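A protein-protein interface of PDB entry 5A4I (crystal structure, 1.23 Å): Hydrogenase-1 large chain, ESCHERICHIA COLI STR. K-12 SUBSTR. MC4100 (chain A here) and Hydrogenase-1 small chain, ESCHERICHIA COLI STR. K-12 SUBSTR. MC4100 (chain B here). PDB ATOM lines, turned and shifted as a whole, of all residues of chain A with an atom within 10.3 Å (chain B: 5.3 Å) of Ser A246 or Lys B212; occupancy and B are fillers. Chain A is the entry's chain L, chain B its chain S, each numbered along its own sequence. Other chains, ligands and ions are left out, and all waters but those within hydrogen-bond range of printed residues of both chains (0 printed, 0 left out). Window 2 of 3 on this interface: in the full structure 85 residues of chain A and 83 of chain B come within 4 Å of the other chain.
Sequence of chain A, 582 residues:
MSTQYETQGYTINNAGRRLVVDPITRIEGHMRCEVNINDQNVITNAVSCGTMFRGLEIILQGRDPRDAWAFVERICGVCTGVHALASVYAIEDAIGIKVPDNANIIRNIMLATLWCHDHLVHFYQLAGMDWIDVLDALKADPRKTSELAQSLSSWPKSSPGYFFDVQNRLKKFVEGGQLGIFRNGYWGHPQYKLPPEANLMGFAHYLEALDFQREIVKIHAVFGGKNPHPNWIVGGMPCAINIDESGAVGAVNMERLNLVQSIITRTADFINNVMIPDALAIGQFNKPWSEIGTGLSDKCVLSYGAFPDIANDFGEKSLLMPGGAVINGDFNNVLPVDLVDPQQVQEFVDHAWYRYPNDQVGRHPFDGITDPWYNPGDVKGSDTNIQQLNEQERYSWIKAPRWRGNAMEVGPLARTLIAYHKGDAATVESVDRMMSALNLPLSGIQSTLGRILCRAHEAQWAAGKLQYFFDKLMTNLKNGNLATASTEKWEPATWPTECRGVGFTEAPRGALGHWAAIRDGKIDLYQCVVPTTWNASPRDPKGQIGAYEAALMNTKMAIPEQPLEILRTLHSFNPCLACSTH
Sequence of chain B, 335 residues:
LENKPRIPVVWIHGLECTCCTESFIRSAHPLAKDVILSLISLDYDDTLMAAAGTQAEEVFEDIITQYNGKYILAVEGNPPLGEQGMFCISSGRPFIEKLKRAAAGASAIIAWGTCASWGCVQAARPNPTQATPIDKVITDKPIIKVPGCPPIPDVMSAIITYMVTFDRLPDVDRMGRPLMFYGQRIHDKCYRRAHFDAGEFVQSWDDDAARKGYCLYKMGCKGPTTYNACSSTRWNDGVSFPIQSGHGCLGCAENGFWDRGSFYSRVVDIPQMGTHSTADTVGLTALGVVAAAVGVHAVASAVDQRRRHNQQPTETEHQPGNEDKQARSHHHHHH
O of Gly A247 lies close to O of Arg B211 (3.5 Å).
The backbone carbonyl oxygen (O) of Arg B211 lies within hydrogen-bond range of the side-chain amide nitrogen (ND2) of Asn A242, at 2.9 Å.
N of Gly B213 sits close to O of Gly A250, at 3.5 Å.
ND2 of Asn A242 sits close to N of Ala A248.
OD1 of Asn A242 is in hydrogen-bond range of N of Asp A244, at 3.4 Å.
The side-chain amide nitrogen (ND2) of Asn A242 is in hydrogen-bond range of the backbone carbonyl oxygen (O) of Ser A246 (3.2 Å).
The backbone carbonyl oxygen (O) of Ala A240 is in hydrogen-bond range of the backbone NH (N) of Val A252 (2.9 Å).
N of Asn A242 sits at hydrogen-bond distance from O of Val A252, at 3.0 Å.
The backbone NH of Glu A245 lies within hydrogen-bond range of the side-chain amide oxygen of Asn A242 (3.0 Å).
CB of Ala A240 touches O of Ala B210, at 3.8 Å.
Arg B211 touches Ala A240.
Arg B211 touches Ile A241.
Ser A246 touches Lys B212 (O to CG, 3.9 Å).
Gly A247 touches Lys B212.
Gly A250 touches Lys B212 (CA to O, 3.99 Å).
Ala A251 touches Arg B211 (CB to O, 3.7 Å).
Arg B211 touches Leu A482.
Ser A246 touches one residue of chain B.
Printed residues of chain B within 4 Å of Gly A247: Arg B211 and Lys B212.
Of the printed residues of chain B, Ala A251 touches Arg B211.
Val A252 touches none of the printed residues of chain B.
Printed residues of chain B within 4 Å of Leu A482: Arg B211 (3.95 Å).
Of the printed residues of chain A, Ala B210 touches Ala A240.
Printed residues of chain A within 4 Å of Arg B211: Ala A240 (3.98 Å), Ile A241 (3.7 Å), Asn A242 (2.9 Å), Gly A247 (3.5 Å), Ala A251 (3.7 Å) and Leu A482 (3.95 Å).
Of the printed residues of chain A, Lys B212 touches Ser A246 (3.9 Å), Gly A247 (3.6 Å) and Gly A250 (3.99 Å).
Of chain A, only Gly A250 (3.2 Å) comes within 4 Å of Gly B213.
No residue of chain A comes within 4 Å of Tyr B214.
The nearest residue of chain B that does not touch Ser A246 is Arg B211 (4.7 Å).
Along chain A the printed residues that touch a printed residue of chain B span positions 240 to 482.
Of the 8 printed residues of chain B, 4 touch a printed residue of chain A.
Printed residues of chain B that touch a printed residue of chain A: Ala B210, Arg B211, Lys B212 and Gly B213.
Among the printed residues, no Asp or Glu carboxylate lies within 4 Å of a Lys or Arg side-chain nitrogen of the other chain.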
ATOM      1  N   PRO A 238      24.610   0.190   4.589  1.00  0.00           N
ATOM      2  CA  PRO A 238      24.966  -0.923   5.482  1.00  0.00           C
ATOM      3  C   PRO A 238      25.559  -0.496   6.815  1.00  0.00           C
ATOM      4  O   PRO A 238      25.767  -1.353   7.684  1.00  0.00           O
ATOM      5  CB  PRO A 238      25.996  -1.710   4.686  1.00  0.00           C
ATOM      6  CG  PRO A 238      26.451  -0.856   3.622  1.00  0.00           C
ATOM      7  CD  PRO A 238      25.585   0.350   3.506  1.00  0.00           C
ATOM      8  N   CYS A 239      25.805   0.803   6.996  1.00  0.00           N
ATOM      9  CA  CYS A 239      26.445   1.332   8.178  1.00  0.00           C
ATOM     10  C   CYS A 239      25.483   1.536   9.322  1.00  0.00           C
ATOM     11  O   CYS A 239      25.112   2.667   9.687  1.00  0.00           O
ATOM     12  CB  CYS A 239      27.217   2.596   7.807  1.00  0.00           C
ATOM     13  SG  CYS A 239      26.220   3.851   6.989  1.00  0.00           S
ATOM     14  N   ALA A 240      25.120   0.429   9.953  1.00  0.00           N
ATOM     15  CA  ALA A 240      24.207   0.440  11.074  1.00  0.00           C
ATOM     16  C   ALA A 240      24.727   1.363  12.160  1.00  0.00           C
ATOM     17  O   ALA A 240      25.964   1.433  12.414  1.00  0.00           O
ATOM     18  CB  ALA A 240      24.052  -0.975  11.628  1.00  0.00           C
ATOM     19  N   ILE A 241      23.799   2.025  12.849  1.00  0.00           N
ATOM     20  CA  ILE A 241      24.086   2.980  13.874  1.00  0.00           C
ATOM     21  C   ILE A 241      23.775   2.401  15.253  1.00  0.00           C
ATOM     22  O   ILE A 241      22.730   1.770  15.459  1.00  0.00           O
ATOM     23  CB  ILE A 241      23.299   4.303  13.632  1.00  0.00           C
ATOM     24  CG1 ILE A 241      23.673   4.917  12.268  1.00  0.00           C
ATOM     25  CG2 ILE A 241      23.469   5.302  14.809  1.00  0.00           C
ATOM     26  CD1 ILE A 241      22.768   6.043  11.865  1.00  0.00           C
ATOM     27  N   ASN A 242      24.645   2.699  16.225  1.00  0.00           N
ATOM     28  CA  ASN A 242      24.418   2.331  17.613  1.00  0.00           C
ATOM     29  C   ASN A 242      25.178   3.363  18.411  1.00  0.00           C
ATOM     30  O   ASN A 242      26.403   3.406  18.389  1.00  0.00           O
ATOM     31  CB  ASN A 242      24.898   0.920  17.862  1.00  0.00           C
ATOM     32  CG  ASN A 242      24.733   0.473  19.301  1.00  0.00           C
ATOM     33  OD1 ASN A 242      24.391   1.258  20.189  1.00  0.00           O
ATOM     34  ND2 ASN A 242      25.000  -0.793  19.554  1.00  0.00           N
ATOM     35  N   ILE A 243      24.437   4.218  19.103  1.00  0.00           N
ATOM     36  CA  ILE A 243      25.037   5.262  19.917  1.00  0.00           C
ATOM     37  C   ILE A 243      25.192   4.881  21.382  1.00  0.00           C
ATOM     38  O   ILE A 243      26.208   5.228  21.995  1.00  0.00           O
ATOM     39  CB  ILE A 243      24.180   6.570  19.834  1.00  0.00           C
ATOM     40  CG1 ILE A 243      23.929   6.975  18.407  1.00  0.00           C
ATOM     41  CG2 ILE A 243      24.850   7.663  20.622  1.00  0.00           C
ATOM     42  CD1 ILE A 243      25.205   7.129  17.634  1.00  0.00           C
ATOM     43  N   ASP A 244      24.202   4.215  21.956  1.00  0.00           N
ATOM     44  CA  ASP A 244      24.123   4.128  23.429  1.00  0.00           C
ATOM     45  C   ASP A 244      23.817   2.755  23.956  1.00  0.00           C
ATOM     46  O   ASP A 244      23.364   2.620  25.096  1.00  0.00           O
ATOM     47  CB  ASP A 244      23.092   5.184  23.946  1.00  0.00           C
ATOM     48  CG  ASP A 244      23.092   5.389  25.468  1.00  0.00           C
ATOM     49  OD1 ASP A 244      24.170   5.467  26.070  1.00  0.00           O
ATOM     50  OD2 ASP A 244      21.986   5.473  26.071  1.00  0.00           O
ATOM     51  N   GLU A 245      24.071   1.727  23.160  1.00  0.00           N
ATOM     52  CA  GLU A 245      23.854   0.350  23.542  1.00  0.00           C
ATOM     53  C   GLU A 245      25.122  -0.450  23.498  1.00  0.00           C
ATOM     54  O   GLU A 245      26.124  -0.024  22.895  1.00  0.00           O
ATOM     55  CB  GLU A 245      22.762  -0.298  22.653  1.00  0.00           C
ATOM     56  CG  GLU A 245      21.421   0.449  22.700  1.00  0.00           C
ATOM     57  CD  GLU A 245      20.613   0.175  21.462  1.00  0.00           C
ATOM     58  OE1 GLU A 245      20.116  -0.930  21.483  1.00  0.00           O
ATOM     59  OE2 GLU A 245      20.529   1.018  20.477  1.00  0.00           O
ATOM     60  N   SER A 246      25.081  -1.624  24.132  1.00  0.00           N
ATOM     61  CA  SER A 246      26.190  -2.539  24.099  1.00  0.00           C
ATOM     62  C   SER A 246      26.565  -2.825  22.637  1.00  0.00           C
ATOM     63  O   SER A 246      25.682  -2.950  21.752  1.00  0.00           O
ATOM     64  CB  SER A 246      25.846  -3.803  24.836  1.00  0.00           C
ATOM     65  OG  SER A 246      26.966  -4.653  24.874  1.00  0.00           O
ATOM     66  N   GLY A 247      27.842  -2.955  22.386  1.00  0.00           N
ATOM     67  CA  GLY A 247      28.232  -3.243  21.014  1.00  0.00           C
ATOM     68  C   GLY A 247      28.293  -2.054  20.058  1.00  0.00           C
ATOM     69  O   GLY A 247      28.495  -2.257  18.860  1.00  0.00           O
ATOM     70  N   ALA A 248      28.179  -0.833  20.585  1.00  0.00           N
ATOM     71  CA  ALA A 248      28.373   0.364  19.744  1.00  0.00           C
ATOM     72  C   ALA A 248      29.745   0.389  19.098  1.00  0.00           C
ATOM     73  O   ALA A 248      29.885   1.006  18.032  1.00  0.00           O
ATOM     74  CB  ALA A 248      28.103   1.633  20.501  1.00  0.00           C
ATOM     75  N   VAL A 249      30.725  -0.299  19.673  1.00  0.00           N
ATOM     76  CA  VAL A 249      32.029  -0.479  19.057  1.00  0.00           C
ATOM     77  C   VAL A 249      31.966  -1.164  17.706  1.00  0.00           C
ATOM     78  O   VAL A 249      32.917  -1.078  16.939  1.00  0.00           O
ATOM     79  CB  VAL A 249      33.009  -1.253  19.979  1.00  0.00           C
ATOM     80  CG1 VAL A 249      33.362  -0.418  21.222  1.00  0.00           C
ATOM     81  CG2 VAL A 249      32.528  -2.630  20.340  1.00  0.00           C
ATOM     82  N   GLY A 250      30.863  -1.859  17.438  1.00  0.00           N
ATOM     83  CA  GLY A 250      30.659  -2.543  16.172  1.00  0.00           C
ATOM     84  C   GLY A 250      29.855  -1.761  15.154  1.00  0.00           C
ATOM     85  O   GLY A 250      29.413  -2.380  14.170  1.00  0.00           O
ATOM     86  N   ALA A 251      29.613  -0.456  15.342  1.00  0.00           N
ATOM     87  CA  ALA A 251      28.682   0.296  14.528  1.00  0.00           C
ATOM     88  C   ALA A 251      29.091   1.739  14.421  1.00  0.00           C
ATOM     89  O   ALA A 251      30.092   2.167  14.988  1.00  0.00           O
ATOM     90  CB  ALA A 251      27.301   0.192  15.155  1.00  0.00           C
ATOM     91  N   VAL A 252      28.303   2.541  13.700  1.00  0.00           N
ATOM     92  CA  VAL A 252      28.515   3.989  13.696  1.00  0.00           C
ATOM     93  C   VAL A 252      28.049   4.526  15.053  1.00  0.00           C
ATOM     94  O   VAL A 252      26.872   4.487  15.372  1.00  0.00           O
ATOM     95  CB  VAL A 252      27.752   4.648  12.548  1.00  0.00           C
ATOM     96  CG1 VAL A 252      27.877   6.166  12.613  1.00  0.00           C
ATOM     97  CG2 VAL A 252      28.224   4.150  11.202  1.00  0.00           C
ATOM     98  N   ASN A 253      29.021   4.980  15.815  1.00  0.00           N
ATOM     99  CA  ASN A 253      28.840   5.425  17.186  1.00  0.00           C
ATOM    100  C   ASN A 253      29.243   6.909  17.321  1.00  0.00           C
ATOM    101  O   ASN A 253      29.583   7.562  16.325  1.00  0.00           O
ATOM    102  CB  ASN A 253      29.618   4.486  18.103  1.00  0.00           C
ATOM    103  CG  ASN A 253      31.086   4.516  17.823  1.00  0.00           C
ATOM    104  OD1 ASN A 253      31.680   5.567  17.674  1.00  0.00           O
ATOM    105  ND2 ASN A 253      31.696   3.342  17.761  1.00  0.00           N
ATOM    106  N   LEU A 482      17.051   5.638  14.544  1.00  0.00           N
ATOM    107  CA  LEU A 482      18.358   5.093  14.167  1.00  0.00           C
ATOM    108  C   LEU A 482      18.347   4.303  12.861  1.00  0.00           C
ATOM    109  O   LEU A 482      19.421   3.985  12.371  1.00  0.00           O
ATOM    110  CB  LEU A 482      18.889   4.140  15.257  1.00  0.00           C
ATOM    111  CG  LEU A 482      19.647   4.843  16.409  1.00  0.00           C
ATOM    112  CD1 LEU A 482      18.895   5.962  17.084  1.00  0.00           C
ATOM    113  CD2 LEU A 482      20.150   3.819  17.397  1.00  0.00           C
ATOM    114  N   HIS B 195      32.824 -13.338  16.306  1.00  0.00           N
ATOM    115  CA  HIS B 195      31.408 -13.577  16.030  1.00  0.00           C
ATOM    116  C   HIS B 195      31.216 -14.728  15.040  1.00  0.00           C
ATOM    117  O   HIS B 195      30.347 -15.599  15.256  1.00  0.00           O
ATOM    118  CB  HIS B 195      30.750 -12.323  15.543  1.00  0.00           C
ATOM    119  CG  HIS B 195      30.865 -11.189  16.499  1.00  0.00           C
ATOM    120  ND1 HIS B 195      30.415 -11.275  17.788  1.00  0.00           N
ATOM    121  CD2 HIS B 195      31.367  -9.938  16.363  1.00  0.00           C
ATOM    122  CE1 HIS B 195      30.619 -10.125  18.407  1.00  0.00           C
ATOM    123  NE2 HIS B 195      31.179  -9.294  17.552  1.00  0.00           N
ATOM    124  N   ASP B 208      19.518  -6.411  14.915  1.00  0.00           N
ATOM    125  CA  ASP B 208      20.205  -6.154  16.166  1.00  0.00           C
ATOM    126  C   ASP B 208      21.650  -6.618  16.086  1.00  0.00           C
ATOM    127  O   ASP B 208      22.572  -5.965  16.622  1.00  0.00           O
ATOM    128  CB  ASP B 208      19.440  -6.863  17.320  1.00  0.00           C
ATOM    129  CG  ASP B 208      18.158  -6.117  17.717  1.00  0.00           C
ATOM    130  OD1 ASP B 208      17.887  -4.979  17.214  1.00  0.00           O
ATOM    131  OD2 ASP B 208      17.438  -6.640  18.577  1.00  0.00           O
ATOM    132  N   ALA B 209      21.871  -7.718  15.394  1.00  0.00           N
ATOM    133  CA  ALA B 209      23.231  -8.226  15.168  1.00  0.00           C
ATOM    134  C   ALA B 209      24.096  -7.211  14.416  1.00  0.00           C
ATOM    135  O   ALA B 209      25.273  -6.983  14.766  1.00  0.00           O
ATOM    136  CB  ALA B 209      23.150  -9.523  14.387  1.00  0.00           C
ATOM    137  N   ALA B 210      23.528  -6.583  13.388  1.00  0.00           N
ATOM    138  CA  ALA B 210      24.293  -5.569  12.650  1.00  0.00           C
ATOM    139  C   ALA B 210      24.692  -4.429  13.533  1.00  0.00           C
ATOM    140  O   ALA B 210      25.779  -3.877  13.385  1.00  0.00           O
ATOM    141  CB  ALA B 210      23.478  -5.028  11.469  1.00  0.00           C
ATOM    142  N   ARG B 211      23.793  -4.013  14.419  1.00  0.00           N
ATOM    143  CA  ARG B 211      24.046  -2.899  15.321  1.00  0.00           C
ATOM    144  C   ARG B 211      25.042  -3.227  16.427  1.00  0.00           C
ATOM    145  O   ARG B 211      25.474  -2.288  17.114  1.00  0.00           O
ATOM    146  CB  ARG B 211      22.737  -2.396  15.901  1.00  0.00           C
ATOM    147  CG  ARG B 211      21.853  -1.730  14.855  1.00  0.00           C
ATOM    148  CD  ARG B 211      20.503  -1.399  15.430  1.00  0.00           C
ATOM    149  NE  ARG B 211      19.644  -0.805  14.400  1.00  0.00           N
ATOM    150  CZ  ARG B 211      18.558  -0.059  14.637  1.00  0.00           C
ATOM    151  NH1 ARG B 211      18.152   0.177  15.864  1.00  0.00           N
ATOM    152  NH2 ARG B 211      17.898   0.453  13.624  1.00  0.00           N
ATOM    153  N   LYS B 212      25.449  -4.504  16.563  1.00  0.00           N
ATOM    154  CA  LYS B 212      26.504  -4.910  17.473  1.00  0.00           C
ATOM    155  C   LYS B 212      27.781  -5.349  16.754  1.00  0.00           C
ATOM    156  O   LYS B 212      28.719  -5.809  17.388  1.00  0.00           O
ATOM    157  CB  LYS B 212      26.010  -6.111  18.318  1.00  0.00           C
ATOM    158  CG  LYS B 212      24.806  -5.819  19.204  1.00  0.00           C
ATOM    159  CD  LYS B 212      24.429  -7.052  19.987  1.00  0.00           C
ATOM    160  CE  LYS B 212      23.689  -8.070  19.190  1.00  0.00           C
ATOM    161  NZ  LYS B 212      23.167  -9.087  20.157  1.00  0.00           N
ATOM    162  N   GLY B 213      27.828  -5.193  15.437  1.00  0.00           N
ATOM    163  CA  GLY B 213      29.005  -5.547  14.670  1.00  0.00           C
ATOM    164  C   GLY B 213      29.254  -7.018  14.512  1.00  0.00           C
ATOM    165  O   GLY B 213      30.386  -7.449  14.468  1.00  0.00           O
ATOM    166  N   TYR B 214      28.174  -7.820  14.409  1.00  0.00           N
ATOM    167  CA  TYR B 214      28.368  -9.253  14.206  1.00  0.00           C
ATOM    168  C   TYR B 214      28.882  -9.559  12.804  1.00  0.00           C
ATOM    169  O   TYR B 214      28.972  -8.702  11.920  1.00  0.00           O
ATOM    170  CB  TYR B 214      27.032  -9.989  14.495  1.00  0.00           C
ATOM    171  CG  TYR B 214      26.709 -10.189  15.952  1.00  0.00           C
ATOM    172  CD1 TYR B 214      27.414  -9.565  16.978  1.00  0.00           C
ATOM    173  CD2 TYR B 214      25.627 -10.994  16.291  1.00  0.00           C
ATOM    174  CE1 TYR B 214      27.072  -9.766  18.321  1.00  0.00           C
ATOM    175  CE2 TYR B 214      25.285 -11.175  17.618  1.00  0.00           C
ATOM    176  CZ  TYR B 214      25.992 -10.545  18.609  1.00  0.00           C
ATOM    177  OH  TYR B 214      25.655 -10.768  19.946  1.00  0.00           O
